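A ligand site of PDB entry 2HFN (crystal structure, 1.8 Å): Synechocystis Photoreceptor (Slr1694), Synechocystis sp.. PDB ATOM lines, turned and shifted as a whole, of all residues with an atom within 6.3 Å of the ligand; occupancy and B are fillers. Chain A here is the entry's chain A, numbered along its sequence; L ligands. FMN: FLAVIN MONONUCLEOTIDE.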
ATOM      1  N   TYR A  11      -5.395  -0.990 -27.504  1.00  0.00           N
ATOM      2  CA  TYR A  11      -4.897  -0.337 -26.302  1.00  0.00           C
ATOM      3  C   TYR A  11      -5.280  -1.105 -25.063  1.00  0.00           C
ATOM      4  O   TYR A  11      -6.174  -1.971 -25.103  1.00  0.00           O
ATOM      5  CB  TYR A  11      -5.422   1.104 -26.208  1.00  0.00           C
ATOM      6  CG  TYR A  11      -6.864   1.170 -25.747  1.00  0.00           C
ATOM      7  CD1 TYR A  11      -7.913   1.118 -26.649  1.00  0.00           C
ATOM      8  CD2 TYR A  11      -7.164   1.205 -24.376  1.00  0.00           C
ATOM      9  CE1 TYR A  11      -9.256   1.154 -26.215  1.00  0.00           C
ATOM     10  CE2 TYR A  11      -8.506   1.228 -23.920  1.00  0.00           C
ATOM     11  CZ  TYR A  11      -9.535   1.178 -24.837  1.00  0.00           C
ATOM     12  OH  TYR A  11     -10.839   1.201 -24.368  1.00  0.00           O
ATOM     13  N   SER A  13      -5.880  -0.373 -20.596  1.00  0.00           N
ATOM     14  CA  SER A  13      -6.098   0.669 -19.587  1.00  0.00           C
ATOM     15  C   SER A  13      -6.385  -0.010 -18.246  1.00  0.00           C
ATOM     16  O   SER A  13      -6.590  -1.239 -18.200  1.00  0.00           O
ATOM     17  CB  SER A  13      -7.293   1.539 -19.947  1.00  0.00           C
ATOM     18  OG  SER A  13      -8.482   0.749 -19.999  1.00  0.00           O
ATOM     19  N   ASP A  26     -23.061  -1.606 -19.171  1.00  0.00           N
ATOM     20  CA  ASP A  26     -23.235  -0.200 -19.573  1.00  0.00           C
ATOM     21  C   ASP A  26     -22.264   0.198 -20.709  1.00  0.00           C
ATOM     22  O   ASP A  26     -22.668   0.838 -21.696  1.00  0.00           O
ATOM     23  CB  ASP A  26     -23.037   0.761 -18.380  1.00  0.00           C
ATOM     24  CG  ASP A  26     -24.161   0.677 -17.349  1.00  0.00           C
ATOM     25  OD1 ASP A  26     -23.892   1.006 -16.168  1.00  0.00           O
ATOM     26  OD2 ASP A  26     -25.315   0.336 -17.707  1.00  0.00           O
ATOM     27  N   ILE A  27     -20.987  -0.165 -20.532  1.00  0.00           N
ATOM     28  CA  ILE A  27     -19.938   0.059 -21.534  1.00  0.00           C
ATOM     29  C   ILE A  27     -20.332  -0.601 -22.855  1.00  0.00           C
ATOM     30  O   ILE A  27     -20.295   0.041 -23.929  1.00  0.00           O
ATOM     31  CB  ILE A  27     -18.551  -0.473 -21.046  1.00  0.00           C
ATOM     32  CG1 ILE A  27     -18.039   0.406 -19.884  1.00  0.00           C
ATOM     33  CG2 ILE A  27     -17.547  -0.480 -22.195  1.00  0.00           C
ATOM     34  CD1 ILE A  27     -16.917  -0.227 -19.043  1.00  0.00           C
ATOM     35  N   GLU A  29     -23.331  -1.611 -23.927  1.00  0.00           N
ATOM     36  CA  GLU A  29     -24.543  -0.979 -24.428  1.00  0.00           C
ATOM     37  C   GLU A  29     -24.210   0.312 -25.158  1.00  0.00           C
ATOM     38  O   GLU A  29     -24.687   0.546 -26.261  1.00  0.00           O
ATOM     39  CB  GLU A  29     -25.530  -0.745 -23.300  1.00  0.00           C
ATOM     40  CG  GLU A  29     -26.079  -2.041 -22.766  1.00  0.00           C
ATOM     41  CD  GLU A  29     -27.264  -1.859 -21.835  1.00  0.00           C
ATOM     42  OE1 GLU A  29     -27.462  -0.757 -21.269  1.00  0.00           O
ATOM     43  OE2 GLU A  29     -27.984  -2.855 -21.668  1.00  0.00           O
ATOM     44  N   SER A  30     -23.361   1.127 -24.530  1.00  0.00           N
ATOM     45  CA  SER A  30     -22.870   2.389 -25.103  1.00  0.00           C
ATOM     46  C   SER A  30     -22.154   2.176 -26.429  1.00  0.00           C
ATOM     47  O   SER A  30     -22.464   2.829 -27.443  1.00  0.00           O
ATOM     48  CB  SER A  30     -21.937   3.109 -24.111  1.00  0.00           C
ATOM     49  OG  SER A  30     -22.716   3.770 -23.104  1.00  0.00           O
ATOM     50  N   SER A  31     -21.207   1.224 -26.440  1.00  0.00           N
ATOM     51  CA  SER A  31     -20.421   0.962 -27.634  1.00  0.00           C
ATOM     52  C   SER A  31     -21.307   0.415 -28.792  1.00  0.00           C
ATOM     53  O   SER A  31     -21.143   0.800 -29.950  1.00  0.00           O
ATOM     54  CB  SER A  31     -19.269   0.006 -27.284  1.00  0.00           C
ATOM     55  OG  SER A  31     -19.771  -1.247 -26.922  1.00  0.00           O
ATOM     56  N   GLN A  32     -22.265  -0.447 -28.466  1.00  0.00           N
ATOM     57  CA  GLN A  32     -23.146  -1.014 -29.482  1.00  0.00           C
ATOM     58  C   GLN A  32     -24.136   0.025 -30.025  1.00  0.00           C
ATOM     59  O   GLN A  32     -24.622  -0.103 -31.145  1.00  0.00           O
ATOM     60  CB  GLN A  32     -23.833  -2.290 -28.966  1.00  0.00           C
ATOM     61  CG  GLN A  32     -22.833  -3.459 -28.806  1.00  0.00           C
ATOM     62  CD  GLN A  32     -23.470  -4.794 -28.479  1.00  0.00           C
ATOM     63  OE1 GLN A  32     -22.880  -5.848 -28.740  1.00  0.00           O
ATOM     64  NE2 GLN A  32     -24.662  -4.757 -27.888  1.00  0.00           N
ATOM     65  N   ARG A  33     -24.428   1.061 -29.227  1.00  0.00           N
ATOM     66  CA  ARG A  33     -25.221   2.218 -29.666  1.00  0.00           C
ATOM     67  C   ARG A  33     -24.481   3.123 -30.657  1.00  0.00           C
ATOM     68  O   ARG A  33     -25.060   3.603 -31.648  1.00  0.00           O
ATOM     69  CB  ARG A  33     -25.601   3.033 -28.449  1.00  0.00           C
ATOM     70  CG  ARG A  33     -26.637   4.099 -28.639  1.00  0.00           C
ATOM     71  CD  ARG A  33     -27.014   4.692 -27.284  1.00  0.00           C
ATOM     72  NE  ARG A  33     -27.401   3.635 -26.349  1.00  0.00           N
ATOM     73  CZ  ARG A  33     -26.912   3.495 -25.119  1.00  0.00           C
ATOM     74  NH1 ARG A  33     -26.033   4.351 -24.630  1.00  0.00           N
ATOM     75  NH2 ARG A  33     -27.335   2.500 -24.353  1.00  0.00           N
ATOM     76  N   ASN A  34     -23.203   3.405 -30.359  1.00  0.00           N
ATOM     77  CA  ASN A  34     -22.426   4.409 -31.086  1.00  0.00           C
ATOM     78  C   ASN A  34     -21.625   3.847 -32.272  1.00  0.00           C
ATOM     79  O   ASN A  34     -21.524   4.483 -33.347  1.00  0.00           O
ATOM     80  CB  ASN A  34     -21.456   5.133 -30.140  1.00  0.00           C
ATOM     81  CG  ASN A  34     -22.137   5.784 -28.967  1.00  0.00           C
ATOM     82  OD1 ASN A  34     -23.273   6.232 -29.070  1.00  0.00           O
ATOM     83  ND2 ASN A  34     -21.446   5.840 -27.840  1.00  0.00           N
ATOM     84  N   ASN A  35     -21.045   2.668 -32.070  1.00  0.00           N
ATOM     85  CA  ASN A  35     -20.111   2.092 -33.056  1.00  0.00           C
ATOM     86  C   ASN A  35     -20.662   1.886 -34.466  1.00  0.00           C
ATOM     87  O   ASN A  35     -19.969   2.238 -35.441  1.00  0.00           O
ATOM     88  CB  ASN A  35     -19.432   0.808 -32.512  1.00  0.00           C
ATOM     89  CG  ASN A  35     -18.362   1.112 -31.468  1.00  0.00           C
ATOM     90  OD1 ASN A  35     -18.116   2.278 -31.143  1.00  0.00           O
ATOM     91  ND2 ASN A  35     -17.698   0.081 -30.961  1.00  0.00           N
ATOM     92  N   ASN A  38     -20.690   4.894 -36.693  1.00  0.00           N
ATOM     93  CA  ASN A  38     -19.293   5.277 -36.877  1.00  0.00           C
ATOM     94  C   ASN A  38     -18.471   4.233 -37.645  1.00  0.00           C
ATOM     95  O   ASN A  38     -17.297   4.455 -37.897  1.00  0.00           O
ATOM     96  CB  ASN A  38     -18.653   5.592 -35.516  1.00  0.00           C
ATOM     97  CG  ASN A  38     -19.194   6.877 -34.916  1.00  0.00           C
ATOM     98  OD1 ASN A  38     -19.557   7.807 -35.645  1.00  0.00           O
ATOM     99  ND2 ASN A  38     -19.283   6.930 -33.582  1.00  0.00           N
ATOM    100  N   ILE A  40     -17.446   1.346 -36.601  1.00  0.00           N
ATOM    101  CA  ILE A  40     -16.408   0.763 -35.715  1.00  0.00           C
ATOM    102  C   ILE A  40     -16.798  -0.685 -35.428  1.00  0.00           C
ATOM    103  O   ILE A  40     -17.992  -0.986 -35.241  1.00  0.00           O
ATOM    104  CB  ILE A  40     -16.242   1.587 -34.400  1.00  0.00           C
ATOM    105  CG1 ILE A  40     -15.800   3.023 -34.707  1.00  0.00           C
ATOM    106  CG2 ILE A  40     -15.308   0.887 -33.321  1.00  0.00           C
ATOM    107  CD1 ILE A  40     -14.418   3.155 -35.307  1.00  0.00           C
ATOM    108  N   LEU A  44     -13.534  -6.125 -26.736  1.00  0.00           N
ATOM    109  CA  LEU A  44     -13.059  -5.587 -25.475  1.00  0.00           C
ATOM    110  C   LEU A  44     -12.945  -6.776 -24.532  1.00  0.00           C
ATOM    111  O   LEU A  44     -13.908  -7.566 -24.420  1.00  0.00           O
ATOM    112  CB  LEU A  44     -14.054  -4.565 -24.920  1.00  0.00           C
ATOM    113  CG  LEU A  44     -13.838  -3.991 -23.504  1.00  0.00           C
ATOM    114  CD1 LEU A  44     -12.573  -3.178 -23.415  1.00  0.00           C
ATOM    115  CD2 LEU A  44     -15.018  -3.153 -23.022  1.00  0.00           C
ATOM    116  N   PHE A  51      -8.422  -3.386 -18.777  1.00  0.00           N
ATOM    117  CA  PHE A  51      -9.096  -3.573 -20.065  1.00  0.00           C
ATOM    118  C   PHE A  51      -8.041  -3.727 -21.197  1.00  0.00           C
ATOM    119  O   PHE A  51      -6.956  -3.147 -21.131  1.00  0.00           O
ATOM    120  CB  PHE A  51      -9.928  -2.343 -20.398  1.00  0.00           C
ATOM    121  CG  PHE A  51     -11.187  -2.165 -19.556  1.00  0.00           C
ATOM    122  CD1 PHE A  51     -11.259  -1.157 -18.592  1.00  0.00           C
ATOM    123  CD2 PHE A  51     -12.316  -2.965 -19.770  1.00  0.00           C
ATOM    124  CE1 PHE A  51     -12.431  -0.962 -17.867  1.00  0.00           C
ATOM    125  CE2 PHE A  51     -13.483  -2.779 -19.046  1.00  0.00           C
ATOM    126  CZ  PHE A  51     -13.551  -1.779 -18.093  1.00  0.00           C
ATOM    127  N   GLN A  53      -8.582  -3.568 -25.546  1.00  0.00           N
ATOM    128  CA  GLN A  53      -9.619  -3.401 -26.580  1.00  0.00           C
ATOM    129  C   GLN A  53      -8.961  -3.233 -27.919  1.00  0.00           C
ATOM    130  O   GLN A  53      -7.854  -2.625 -28.029  1.00  0.00           O
ATOM    131  CB  GLN A  53     -10.526  -2.170 -26.301  1.00  0.00           C
ATOM    132  CG  GLN A  53     -11.763  -2.127 -27.226  1.00  0.00           C
ATOM    133  CD  GLN A  53     -12.716  -0.978 -26.895  1.00  0.00           C
ATOM    134  OE1 GLN A  53     -12.298   0.070 -26.393  1.00  0.00           O
ATOM    135  NE2 GLN A  53     -14.000  -1.183 -27.153  1.00  0.00           N
ATOM    136  N   LEU A  55     -10.011  -1.760 -31.786  1.00  0.00           N
ATOM    137  CA  LEU A  55     -10.979  -0.987 -32.547  1.00  0.00           C
ATOM    138  C   LEU A  55     -10.525  -1.024 -34.006  1.00  0.00           C
ATOM    139  O   LEU A  55      -9.308  -0.879 -34.293  1.00  0.00           O
ATOM    140  CB  LEU A  55     -10.969   0.479 -32.049  1.00  0.00           C
ATOM    141  CG  LEU A  55     -11.330   0.728 -30.583  1.00  0.00           C
ATOM    142  CD1 LEU A  55     -10.953   2.158 -30.127  1.00  0.00           C
ATOM    143  CD2 LEU A  55     -12.815   0.503 -30.389  1.00  0.00           C
ATOM    144  N   THR A  65     -13.407   7.869 -31.829  1.00  0.00           N
ATOM    145  CA  THR A  65     -13.896   6.910 -30.850  1.00  0.00           C
ATOM    146  C   THR A  65     -12.888   6.705 -29.718  1.00  0.00           C
ATOM    147  O   THR A  65     -13.245   6.789 -28.532  1.00  0.00           O
ATOM    148  CB  THR A  65     -14.284   5.575 -31.541  1.00  0.00           C
ATOM    149  OG1 THR A  65     -15.324   5.829 -32.486  1.00  0.00           O
ATOM    150  CG2 THR A  65     -14.777   4.566 -30.559  1.00  0.00           C
ATOM    151  N   ARG A  68     -12.488   9.738 -27.369  1.00  0.00           N
ATOM    152  CA  ARG A  68     -13.715   9.820 -26.560  1.00  0.00           C
ATOM    153  C   ARG A  68     -13.650   8.785 -25.410  1.00  0.00           C
ATOM    154  O   ARG A  68     -13.887   9.125 -24.243  1.00  0.00           O
ATOM    155  CB  ARG A  68     -14.936   9.608 -27.448  1.00  0.00           C
ATOM    156  CG  ARG A  68     -16.282   9.599 -26.747  1.00  0.00           C
ATOM    157  CD  ARG A  68     -17.412   9.918 -27.750  1.00  0.00           C
ATOM    158  NE  ARG A  68     -17.382   9.068 -28.956  1.00  0.00           N
ATOM    159  CZ  ARG A  68     -17.784   7.803 -28.987  1.00  0.00           C
ATOM    160  NH1 ARG A  68     -18.219   7.225 -27.877  1.00  0.00           N
ATOM    161  NH2 ARG A  68     -17.759   7.111 -30.126  1.00  0.00           N
ATOM    162  N   ILE A  69     -13.284   7.547 -25.757  1.00  0.00           N
ATOM    163  CA  ILE A  69     -13.089   6.466 -24.781  1.00  0.00           C
ATOM    164  C   ILE A  69     -12.083   6.881 -23.690  1.00  0.00           C
ATOM    165  O   ILE A  69     -12.324   6.623 -22.502  1.00  0.00           O
ATOM    166  CB  ILE A  69     -12.620   5.105 -25.447  1.00  0.00           C
ATOM    167  CG1 ILE A  69     -13.739   4.483 -26.319  1.00  0.00           C
ATOM    168  CG2 ILE A  69     -12.212   4.117 -24.368  1.00  0.00           C
ATOM    169  CD1 ILE A  69     -13.251   3.292 -27.187  1.00  0.00           C
ATOM    170  N   VAL A  70     -10.961   7.519 -24.057  1.00  0.00           N
ATOM    171  CA  VAL A  70     -10.015   7.931 -22.976  1.00  0.00           C
ATOM    172  C   VAL A  70     -10.617   8.918 -21.949  1.00  0.00           C
ATOM    173  O   VAL A  70     -10.161   8.989 -20.802  1.00  0.00           O
ATOM    174  CB  VAL A  70      -8.513   8.269 -23.390  1.00  0.00           C
ATOM    175  CG1 VAL A  70      -8.119   7.821 -24.794  1.00  0.00           C
ATOM    176  CG2 VAL A  70      -8.059   9.679 -22.977  1.00  0.00           C
ATOM    177  N   GLN A  71     -11.665   9.624 -22.350  1.00  0.00           N
ATOM    178  CA  GLN A  71     -12.348  10.568 -21.450  1.00  0.00           C
ATOM    179  C   GLN A  71     -13.281   9.893 -20.423  1.00  0.00           C
ATOM    180  O   GLN A  71     -13.823  10.560 -19.539  1.00  0.00           O
ATOM    181  CB  GLN A  71     -13.090  11.622 -22.280  1.00  0.00           C
ATOM    182  CG  GLN A  71     -12.145  12.545 -23.033  1.00  0.00           C
ATOM    183  CD  GLN A  71     -11.120  13.189 -22.135  1.00  0.00           C
ATOM    184  OE1 GLN A  71     -11.462  13.906 -21.175  1.00  0.00           O
ATOM    185  NE2 GLN A  71      -9.842  12.945 -22.420  1.00  0.00           N
ATOM    186  N   ASP A  72     -13.436   8.578 -20.536  1.00  0.00           N
ATOM    187  CA  ASP A  72     -14.345   7.823 -19.662  1.00  0.00           C
ATOM    188  C   ASP A  72     -13.798   7.705 -18.240  1.00  0.00           C
ATOM    189  O   ASP A  72     -12.666   7.235 -18.045  1.00  0.00           O
ATOM    190  CB  ASP A  72     -14.638   6.432 -20.236  1.00  0.00           C
ATOM    191  CG  ASP A  72     -15.898   5.809 -19.662  1.00  0.00           C
ATOM    192  OD1 ASP A  72     -16.815   5.512 -20.458  1.00  0.00           O
ATOM    193  OD2 ASP A  72     -15.988   5.632 -18.422  1.00  0.00           O
ATOM    194  N   ARG A  74     -14.420   5.673 -16.014  1.00  0.00           N
ATOM    195  CA  ARG A  74     -14.330   4.267 -15.547  1.00  0.00           C
ATOM    196  C   ARG A  74     -12.967   3.574 -15.781  1.00  0.00           C
ATOM    197  O   ARG A  74     -12.764   2.401 -15.381  1.00  0.00           O
ATOM    198  CB  ARG A  74     -15.466   3.421 -16.135  1.00  0.00           C
ATOM    199  CG  ARG A  74     -16.846   3.793 -15.572  1.00  0.00           C
ATOM    200  CD  ARG A  74     -17.957   3.158 -16.384  1.00  0.00           C
ATOM    201  NE  ARG A  74     -18.041   3.698 -17.738  1.00  0.00           N
ATOM    202  CZ  ARG A  74     -19.104   3.568 -18.535  1.00  0.00           C
ATOM    203  NH1 ARG A  74     -20.192   2.936 -18.102  1.00  0.00           N
ATOM    204  NH2 ARG A  74     -19.094   4.097 -19.752  1.00  0.00           N
ATOM    205  N   HIS A  75     -12.032   4.291 -16.403  1.00  0.00           N
ATOM    206  CA  HIS A  75     -10.661   3.788 -16.584  1.00  0.00           C
ATOM    207  C   HIS A  75      -9.641   4.913 -16.706  1.00  0.00           C
ATOM    208  O   HIS A  75     -10.008   6.088 -16.945  1.00  0.00           O
ATOM    209  CB  HIS A  75     -10.537   2.756 -17.729  1.00  0.00           C
ATOM    210  CG  HIS A  75     -10.796   3.316 -19.104  1.00  0.00           C
ATOM    211  ND1 HIS A  75     -10.398   2.647 -20.237  1.00  0.00           N
ATOM    212  CD2 HIS A  75     -11.408   4.444 -19.522  1.00  0.00           C
ATOM    213  CE1 HIS A  75     -10.753   3.336 -21.305  1.00  0.00           C
ATOM    214  NE2 HIS A  75     -11.369   4.434 -20.910  1.00  0.00           N
ATOM    215  N   SER A  95     -20.184  -4.834 -33.861  1.00  0.00           N
ATOM    216  CA  SER A  95     -19.862  -3.427 -33.577  1.00  0.00           C
ATOM    217  C   SER A  95     -19.015  -3.306 -32.306  1.00  0.00           C
ATOM    218  O   SER A  95     -18.110  -2.484 -32.236  1.00  0.00           O
ATOM    219  CB  SER A  95     -21.130  -2.581 -33.456  1.00  0.00           C
ATOM    220  OG  SER A  95     -21.917  -3.036 -32.381  1.00  0.00           O
ATOM    221  N   MET A  96     -19.367  -4.096 -31.295  1.00  0.00           N
ATOM    222  CA  MET A  96     -18.462  -4.390 -30.183  1.00  0.00           C
ATOM    223  C   MET A  96     -18.884  -5.720 -29.538  1.00  0.00           C
ATOM    224  O   MET A  96     -20.090  -6.033 -29.451  1.00  0.00           O
ATOM    225  CB  MET A  96     -18.472  -3.265 -29.132  1.00  0.00           C
ATOM    226  CG  MET A  96     -17.406  -3.410 -28.002  1.00  0.00           C
ATOM    227  SD  MET A  96     -15.717  -3.738 -28.569  1.00  0.00           S
ATOM    228  CE  MET A  96     -15.543  -2.494 -29.838  1.00  0.00           C
HETATM  229  N1  FMN L   1     -17.885   3.870 -26.483  1.00  0.00           N
HETATM  230  C2  FMN L   1     -18.118   3.646 -27.807  1.00  0.00           C
HETATM  231  O2  FMN L   1     -18.903   4.369 -28.415  1.00  0.00           O
HETATM  232  N3  FMN L   1     -17.436   2.624 -28.480  1.00  0.00           N
HETATM  233  C4  FMN L   1     -16.520   1.826 -27.821  1.00  0.00           C
HETATM  234  O4  FMN L   1     -15.990   0.868 -28.439  1.00  0.00           O
HETATM  235  C4A FMN L   1     -16.302   2.049 -26.454  1.00  0.00           C
HETATM  236  N5  FMN L   1     -15.425   1.256 -25.727  1.00  0.00           N
HETATM  237  C5A FMN L   1     -15.200   1.520 -24.374  1.00  0.00           C
HETATM  238  C6  FMN L   1     -14.262   0.757 -23.668  1.00  0.00           C
HETATM  239  C7  FMN L   1     -14.052   1.011 -22.302  1.00  0.00           C
HETATM  240  C7M FMN L   1     -12.897   0.316 -21.626  1.00  0.00           C
HETATM  241  C8  FMN L   1     -14.773   2.033 -21.642  1.00  0.00           C
HETATM  242  C8M FMN L   1     -14.418   2.447 -20.234  1.00  0.00           C
HETATM  243  C9  FMN L   1     -15.680   2.817 -22.363  1.00  0.00           C
HETATM  244  C9A FMN L   1     -15.905   2.553 -23.717  1.00  0.00           C
HETATM  245  N10 FMN L   1     -16.820   3.310 -24.446  1.00  0.00           N
HETATM  246  C10 FMN L   1     -17.001   3.073 -25.798  1.00  0.00           C
HETATM  247  C1' FMN L   1     -17.886   4.119 -23.729  1.00  0.00           C
HETATM  248  C2' FMN L   1     -17.619   5.628 -23.816  1.00  0.00           C
HETATM  249  O2' FMN L   1     -16.522   5.969 -23.012  1.00  0.00           O
HETATM  250  C3' FMN L   1     -18.841   6.479 -23.388  1.00  0.00           C
HETATM  251  O3' FMN L   1     -19.277   6.020 -22.129  1.00  0.00           O
HETATM  252  C4' FMN L   1     -19.991   6.333 -24.372  1.00  0.00           C
HETATM  253  O4' FMN L   1     -19.549   6.562 -25.685  1.00  0.00           O
HETATM  254  C5' FMN L   1     -21.146   7.311 -24.102  1.00  0.00           C
HETATM  255  O5' FMN L   1     -22.192   6.962 -24.986  1.00  0.00           O
HETATM  256  P   FMN L   1     -23.704   7.003 -24.471  1.00  0.00           P
HETATM  257  O1P FMN L   1     -23.821   8.322 -23.753  1.00  0.00           O
HETATM  258  O2P FMN L   1     -24.002   5.893 -23.510  1.00  0.00           O
HETATM  259  O3P FMN L   1     -24.610   6.849 -25.659  1.00  0.00           O
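O of Ile 69 sits at hydrogen-bond distance from NE2 of His 75 (2.9 Å). ND2 of Asn 38 sits at hydrogen-bond distance from O of Asn 34, at 3.3 Å. The guanidinium group (NH2) of Arg 74 lies within salt-bridge range of the side-chain carboxylate (OD1) of Asp 72 (2.8 Å). The backbone carbonyl oxygen of Ser 95 sits at hydrogen-bond distance from the side-chain amide nitrogen of Asn 35, 2.9 Å away. The side-chain hydroxyl (OG) of Ser 31 lies within hydrogen-bond range of the backbone carbonyl oxygen (O) of Ile 27, at 3.3 Å. O of Ser 13 sits at hydrogen-bond distance from N of Phe 51 (2.9 Å). OG of Ser 13 lies within hydrogen-bond range of ND1 of His 75, at 2.7 Å. The backbone carbonyl oxygen of Met 96 sits close to the side-chain amide oxygen of Gln 32 (2.9 Å).
An oxygen (O4') of the ligand lies within hydrogen-bond range of the guanidinium group (NH1) of Arg 68 (2.6 Å). The guanidinium group of Arg 74 is in hydrogen-bond range of an oxygen (O3') of the ligand. An oxygen (O2P) of the ligand sits at hydrogen-bond distance from the side-chain hydroxyl (OG) of Ser 30. O2' of the ligand is in hydrogen-bond range of OD1 of Asp 72. The guanidinium group of Arg 33 is in salt-bridge range of an oxygen (O2P) of the ligand. NE2 of Gln 53 sits at hydrogen-bond distance from O4 of the ligand (3.1 Å). O4' of the ligand sits at hydrogen-bond distance from ND2 of Asn 34 (3.0 Å). N3 of the ligand lies within hydrogen-bond range of OD1 of Asn 35, 2.8 Å away.
Tyr 11 touches the ligand. Ile 27 touches the ligand (CG2 to C9A, 3.8 Å). CB of Ser 31 touches C4 of the ligand (3.3 Å). CD1 of Leu 44 touches C7M of the ligand, at 3.9 Å. Phe 51 touches the ligand. CD2 of Leu 55 touches O4 of the ligand (3.7 Å). CG2 of Thr 65 touches N3 of the ligand, at 3.9 Å. CD1 of Ile 69 touches N5 of the ligand, at 3.3 Å. His 75 touches the ligand. Met 96 touches the ligand. Of the 27 residues printed, 18 come within 4 Å of the ligand.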
